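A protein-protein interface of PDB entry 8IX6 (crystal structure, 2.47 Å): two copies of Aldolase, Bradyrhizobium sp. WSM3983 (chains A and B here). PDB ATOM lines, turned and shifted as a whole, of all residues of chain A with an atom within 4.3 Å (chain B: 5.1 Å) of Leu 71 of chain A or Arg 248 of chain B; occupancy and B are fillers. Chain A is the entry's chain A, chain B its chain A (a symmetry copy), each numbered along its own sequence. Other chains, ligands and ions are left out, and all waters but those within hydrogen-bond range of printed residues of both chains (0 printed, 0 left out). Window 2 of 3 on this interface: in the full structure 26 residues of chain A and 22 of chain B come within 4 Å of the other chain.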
ATOM      1  N   LEU A  50      29.120  -7.711  22.667  1.00  0.00           N
ATOM      2  CA  LEU A  50      27.747  -7.811  23.139  1.00  0.00           C
ATOM      3  C   LEU A  50      27.664  -7.896  24.658  1.00  0.00           C
ATOM      4  O   LEU A  50      26.664  -8.387  25.194  1.00  0.00           O
ATOM      5  CB  LEU A  50      27.052  -9.012  22.495  1.00  0.00           C
ATOM      6  CG  LEU A  50      27.059  -9.031  20.965  1.00  0.00           C
ATOM      7  CD1 LEU A  50      26.696 -10.410  20.436  1.00  0.00           C
ATOM      8  CD2 LEU A  50      26.115  -7.971  20.413  1.00  0.00           C
ATOM      9  N   LEU A  67      17.268  -5.557  26.364  1.00  0.00           N
ATOM     10  CA  LEU A  67      17.582  -5.674  24.947  1.00  0.00           C
ATOM     11  C   LEU A  67      17.766  -7.138  24.567  1.00  0.00           C
ATOM     12  O   LEU A  67      18.372  -7.917  25.307  1.00  0.00           O
ATOM     13  CB  LEU A  67      18.849  -4.878  24.623  1.00  0.00           C
ATOM     14  CG  LEU A  67      19.402  -4.928  23.199  1.00  0.00           C
ATOM     15  CD1 LEU A  67      18.553  -4.077  22.271  1.00  0.00           C
ATOM     16  CD2 LEU A  67      20.853  -4.466  23.177  1.00  0.00           C
ATOM     17  N   ARG A  68      17.236  -7.508  23.403  1.00  0.00           N
ATOM     18  CA  ARG A  68      17.290  -8.895  22.969  1.00  0.00           C
ATOM     19  C   ARG A  68      18.713  -9.287  22.577  1.00  0.00           C
ATOM     20  O   ARG A  68      19.551  -8.447  22.237  1.00  0.00           O
ATOM     21  CB  ARG A  68      16.334  -9.135  21.799  1.00  0.00           C
ATOM     22  CG  ARG A  68      16.462  -8.139  20.660  1.00  0.00           C
ATOM     23  CD  ARG A  68      15.194  -8.112  19.810  1.00  0.00           C
ATOM     24  NE  ARG A  68      15.480  -7.959  18.388  1.00  0.00           N
ATOM     25  CZ  ARG A  68      16.020  -8.899  17.624  1.00  0.00           C
ATOM     26  NH1 ARG A  68      16.331 -10.090  18.108  1.00  0.00           N
ATOM     27  NH2 ARG A  68      16.252  -8.640  16.341  1.00  0.00           N
ATOM     28  N   PHE A  69      18.970 -10.592  22.628  1.00  0.00           N
ATOM     29  CA  PHE A  69      20.305 -11.125  22.390  1.00  0.00           C
ATOM     30  C   PHE A  69      20.793 -10.786  20.985  1.00  0.00           C
ATOM     31  O   PHE A  69      20.013 -10.694  20.033  1.00  0.00           O
ATOM     32  CB  PHE A  69      20.301 -12.643  22.604  1.00  0.00           C
ATOM     33  CG  PHE A  69      21.468 -13.359  21.976  1.00  0.00           C
ATOM     34  CD1 PHE A  69      22.658 -13.509  22.667  1.00  0.00           C
ATOM     35  CD2 PHE A  69      21.364 -13.910  20.706  1.00  0.00           C
ATOM     36  CE1 PHE A  69      23.730 -14.174  22.099  1.00  0.00           C
ATOM     37  CE2 PHE A  69      22.431 -14.573  20.132  1.00  0.00           C
ATOM     38  CZ  PHE A  69      23.615 -14.707  20.829  1.00  0.00           C
ATOM     39  N   GLY A  70      22.108 -10.593  20.866  1.00  0.00           N
ATOM     40  CA  GLY A  70      22.752 -10.393  19.587  1.00  0.00           C
ATOM     41  C   GLY A  70      22.800  -8.964  19.094  1.00  0.00           C
ATOM     42  O   GLY A  70      23.451  -8.701  18.075  1.00  0.00           O
ATOM     43  N   LEU A  71      22.141  -8.032  19.774  1.00  0.00           N
ATOM     44  CA  LEU A  71      22.078  -6.648  19.329  1.00  0.00           C
ATOM     45  C   LEU A  71      23.023  -5.775  20.143  1.00  0.00           C
ATOM     46  O   LEU A  71      23.134  -5.925  21.364  1.00  0.00           O
ATOM     47  CB  LEU A  71      20.652  -6.105  19.433  1.00  0.00           C
ATOM     48  CG  LEU A  71      19.663  -6.672  18.414  1.00  0.00           C
ATOM     49  CD1 LEU A  71      18.339  -5.937  18.486  1.00  0.00           C
ATOM     50  CD2 LEU A  71      20.243  -6.595  17.010  1.00  0.00           C
ATOM     51  N   GLY A  72      23.711  -4.861  19.450  1.00  0.00           N
ATOM     52  CA  GLY A  72      24.569  -3.898  20.104  1.00  0.00           C
ATOM     53  C   GLY A  72      23.824  -2.640  20.506  1.00  0.00           C
ATOM     54  O   GLY A  72      22.664  -2.435  20.154  1.00  0.00           O
ATOM     55  N   GLU A  75      22.579  -0.015  17.701  1.00  0.00           N
ATOM     56  CA  GLU A  75      21.560  -0.486  16.772  1.00  0.00           C
ATOM     57  C   GLU A  75      20.254  -0.815  17.483  1.00  0.00           C
ATOM     58  O   GLU A  75      19.427  -1.562  16.948  1.00  0.00           O
ATOM     59  CB  GLU A  75      22.059  -1.698  15.982  1.00  0.00           C
ATOM     60  CG  GLU A  75      22.477  -2.888  16.831  1.00  0.00           C
ATOM     61  CD  GLU A  75      23.106  -3.995  16.006  1.00  0.00           C
ATOM     62  OE1 GLU A  75      23.285  -3.801  14.784  1.00  0.00           O
ATOM     63  OE2 GLU A  75      23.417  -5.061  16.576  1.00  0.00           O
ATOM     64  N   ASP A  80      13.125  -3.303  19.937  1.00  0.00           N
ATOM     65  CA  ASP A  80      14.128  -4.317  20.228  1.00  0.00           C
ATOM     66  C   ASP A  80      14.198  -4.678  21.704  1.00  0.00           C
ATOM     67  O   ASP A  80      14.971  -5.567  22.075  1.00  0.00           O
ATOM     68  CB  ASP A  80      15.505  -3.850  19.746  1.00  0.00           C
ATOM     69  CG  ASP A  80      15.644  -3.902  18.237  1.00  0.00           C
ATOM     70  OD1 ASP A  80      15.190  -4.894  17.628  1.00  0.00           O
ATOM     71  OD2 ASP A  80      16.213  -2.954  17.659  1.00  0.00           O
ATOM     72  N   ALA B 241      27.797 -14.666  16.961  1.00  0.00           N
ATOM     73  CA  ALA B 241      26.901 -13.528  17.132  1.00  0.00           C
ATOM     74  C   ALA B 241      27.676 -12.218  17.204  1.00  0.00           C
ATOM     75  O   ALA B 241      27.250 -11.206  16.636  1.00  0.00           O
ATOM     76  CB  ALA B 241      26.045 -13.715  18.383  1.00  0.00           C
ATOM     77  N   ASP B 244      28.747 -11.277  13.708  1.00  0.00           N
ATOM     78  CA  ASP B 244      27.609 -10.733  12.974  1.00  0.00           C
ATOM     79  C   ASP B 244      27.334  -9.290  13.377  1.00  0.00           C
ATOM     80  O   ASP B 244      27.062  -8.438  12.522  1.00  0.00           O
ATOM     81  CB  ASP B 244      26.367 -11.595  13.209  1.00  0.00           C
ATOM     82  CG  ASP B 244      26.495 -12.984  12.607  1.00  0.00           C
ATOM     83  OD1 ASP B 244      27.373 -13.180  11.741  1.00  0.00           O
ATOM     84  OD2 ASP B 244      25.715 -13.879  12.999  1.00  0.00           O
ATOM     85  N   TYR B 245      27.401  -8.999  14.680  1.00  0.00           N
ATOM     86  CA  TYR B 245      27.202  -7.633  15.152  1.00  0.00           C
ATOM     87  C   TYR B 245      28.228  -6.683  14.549  1.00  0.00           C
ATOM     88  O   TYR B 245      27.889  -5.561  14.151  1.00  0.00           O
ATOM     89  CB  TYR B 245      27.273  -7.598  16.679  1.00  0.00           C
ATOM     90  CG  TYR B 245      27.560  -6.227  17.248  1.00  0.00           C
ATOM     91  CD1 TYR B 245      26.651  -5.189  17.099  1.00  0.00           C
ATOM     92  CD2 TYR B 245      28.737  -5.973  17.940  1.00  0.00           C
ATOM     93  CE1 TYR B 245      26.909  -3.935  17.615  1.00  0.00           C
ATOM     94  CE2 TYR B 245      29.002  -4.719  18.464  1.00  0.00           C
ATOM     95  CZ  TYR B 245      28.082  -3.705  18.299  1.00  0.00           C
ATOM     96  OH  TYR B 245      28.333  -2.454  18.815  1.00  0.00           O
ATOM     97  N   TRP B 246      29.489  -7.114  14.477  1.00  0.00           N
ATOM     98  CA  TRP B 246      30.529  -6.274  13.896  1.00  0.00           C
ATOM     99  C   TRP B 246      30.299  -6.057  12.405  1.00  0.00           C
ATOM    100  O   TRP B 246      30.581  -4.974  11.879  1.00  0.00           O
ATOM    101  CB  TRP B 246      31.901  -6.900  14.140  1.00  0.00           C
ATOM    102  CG  TRP B 246      32.387  -6.783  15.551  1.00  0.00           C
ATOM    103  CD1 TRP B 246      32.095  -5.791  16.439  1.00  0.00           C
ATOM    104  CD2 TRP B 246      33.263  -7.689  16.235  1.00  0.00           C
ATOM    105  NE1 TRP B 246      32.731  -6.024  17.636  1.00  0.00           N
ATOM    106  CE2 TRP B 246      33.455  -7.183  17.536  1.00  0.00           C
ATOM    107  CE3 TRP B 246      33.902  -8.879  15.873  1.00  0.00           C
ATOM    108  CZ2 TRP B 246      34.259  -7.824  18.475  1.00  0.00           C
ATOM    109  CZ3 TRP B 246      34.699  -9.514  16.809  1.00  0.00           C
ATOM    110  CH2 TRP B 246      34.870  -8.986  18.094  1.00  0.00           C
ATOM    111  N   CYS B 247      29.796  -7.078  11.707  1.00  0.00           N
ATOM    112  CA  CYS B 247      29.522  -6.940  10.279  1.00  0.00           C
ATOM    113  C   CYS B 247      28.478  -5.862  10.022  1.00  0.00           C
ATOM    114  O   CYS B 247      28.665  -4.991   9.164  1.00  0.00           O
ATOM    115  CB  CYS B 247      29.060  -8.279   9.701  1.00  0.00           C
ATOM    116  SG  CYS B 247      30.373  -9.493   9.478  1.00  0.00           S
ATOM    117  N   ARG B 248      27.369  -5.903  10.765  1.00  0.00           N
ATOM    118  CA  ARG B 248      26.313  -4.907  10.625  1.00  0.00           C
ATOM    119  C   ARG B 248      26.788  -3.498  10.952  1.00  0.00           C
ATOM    120  O   ARG B 248      26.062  -2.536  10.672  1.00  0.00           O
ATOM    121  CB  ARG B 248      25.130  -5.281  11.523  1.00  0.00           C
ATOM    122  CG  ARG B 248      24.540  -6.649  11.212  1.00  0.00           C
ATOM    123  CD  ARG B 248      23.325  -6.967  12.072  1.00  0.00           C
ATOM    124  NE  ARG B 248      23.567  -6.738  13.492  1.00  0.00           N
ATOM    125  CZ  ARG B 248      23.688  -7.700  14.397  1.00  0.00           C
ATOM    126  NH1 ARG B 248      23.629  -8.979  14.061  1.00  0.00           N
ATOM    127  NH2 ARG B 248      23.874  -7.371  15.673  1.00  0.00           N
ATOM    128  N   GLN B 249      27.980  -3.354  11.528  1.00  0.00           N
ATOM    129  CA  GLN B 249      28.513  -2.053  11.896  1.00  0.00           C
ATOM    130  C   GLN B 249      29.344  -1.423  10.792  1.00  0.00           C
ATOM    131  O   GLN B 249      29.550  -0.204  10.808  1.00  0.00           O
ATOM    132  CB  GLN B 249      29.371  -2.182  13.160  1.00  0.00           C
ATOM    133  CG  GLN B 249      28.634  -2.200  14.512  1.00  0.00           C
ATOM    134  CD  GLN B 249      27.663  -1.048  14.755  1.00  0.00           C
ATOM    135  OE1 GLN B 249      27.097  -0.457  13.835  1.00  0.00           O
ATOM    136  NE2 GLN B 249      27.473  -0.729  16.025  1.00  0.00           N
ATOM    137  N   THR B 250      29.827  -2.219   9.844  1.00  0.00           N
ATOM    138  CA  THR B 250      30.685  -1.720   8.781  1.00  0.00           C
ATOM    139  C   THR B 250      29.868  -0.992   7.721  1.00  0.00           C
ATOM    140  O   THR B 250      28.680  -1.262   7.548  1.00  0.00           O
ATOM    141  CB  THR B 250      31.477  -2.862   8.123  1.00  0.00           C
ATOM    142  OG1 THR B 250      30.562  -3.816   7.569  1.00  0.00           O
ATOM    143  CG2 THR B 250      32.349  -3.555   9.157  1.00  0.00           C
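OE2 of Glu 75 of chain A lies within salt-bridge range of NH2 of Arg 248 of chain B. O of Gly 70 of chain A is in hydrogen-bond range of NH2 of Arg 248 of chain B, at 2.8 Å.
The side-chain amide nitrogen (NE2) of Gln 249 of chain B sits at hydrogen-bond distance from the side-chain hydroxyl (OH) of Tyr 245 of chain B. The side-chain carboxylate (OE2) of Glu 75 of chain A is in hydrogen-bond range of the backbone NH (N) of Gly 72 of chain A.
Among the printed residues, pairs that only touch across the chains: Glu 75 of chain A with Tyr 245 of chain B (3.3 Å), Gly 72 of chain A with Tyr 245 of chain B (3.4 Å), Phe 69 of chain A with Ala 241 of chain B (3.6 Å), Leu 50 of chain A with Ala 241 of chain B (3.8 Å), Leu 50 of chain A with Tyr 245 of chain B (3.9 Å) and Leu 71 of chain A with Arg 248 of chain B (3.9 Å).
Printed residues of chain B within 4 Å of Leu 71 of chain A: Arg 248. Of the printed residues of chain A, Tyr 245 of chain B touches Leu 50 (3.9 Å), Gly 72 (3.4 Å) and Glu 75 (3.3 Å). Printed residues of chain B within 4 Å of Gly 70 of chain A: Arg 248 (2.8 Å). Printed residues of chain B within 4 Å of Leu 50 of chain A: Ala 241 and Tyr 245. Printed residues of chain B within 4 Å of Gly 72 of chain A: Tyr 245 (3.4 Å). Gln 249 of chain B touches none of the printed residues of chain A. The nearest residue of chain B that does not touch Leu 71 of chain A is Tyr 245 of chain B (4.8 Å).
Of the 9 printed residues of chain A, 6 touch a printed residue of chain B. Hydrophobic or aromatic side chains of chain A within 4 Å of the printed part of chain B: Leu 50, Phe 69 and Leu 71. Along chain A the printed residues that touch a printed residue of chain B span positions 50 to 75. Printed residues of chain B that touch a printed residue of chain A: Ala 241, Tyr 245 and Arg 248. Hydrophobic or aromatic side chains of chain B that line the printed part of chain A: Ala 241 and Tyr 245. Among the printed residues, Asp or Glu carboxylates within 4 Å of a Lys or Arg side-chain nitrogen of the other chain: Glu 75 of chain A with Arg 248 of chain B.
No position is printed for both chains.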
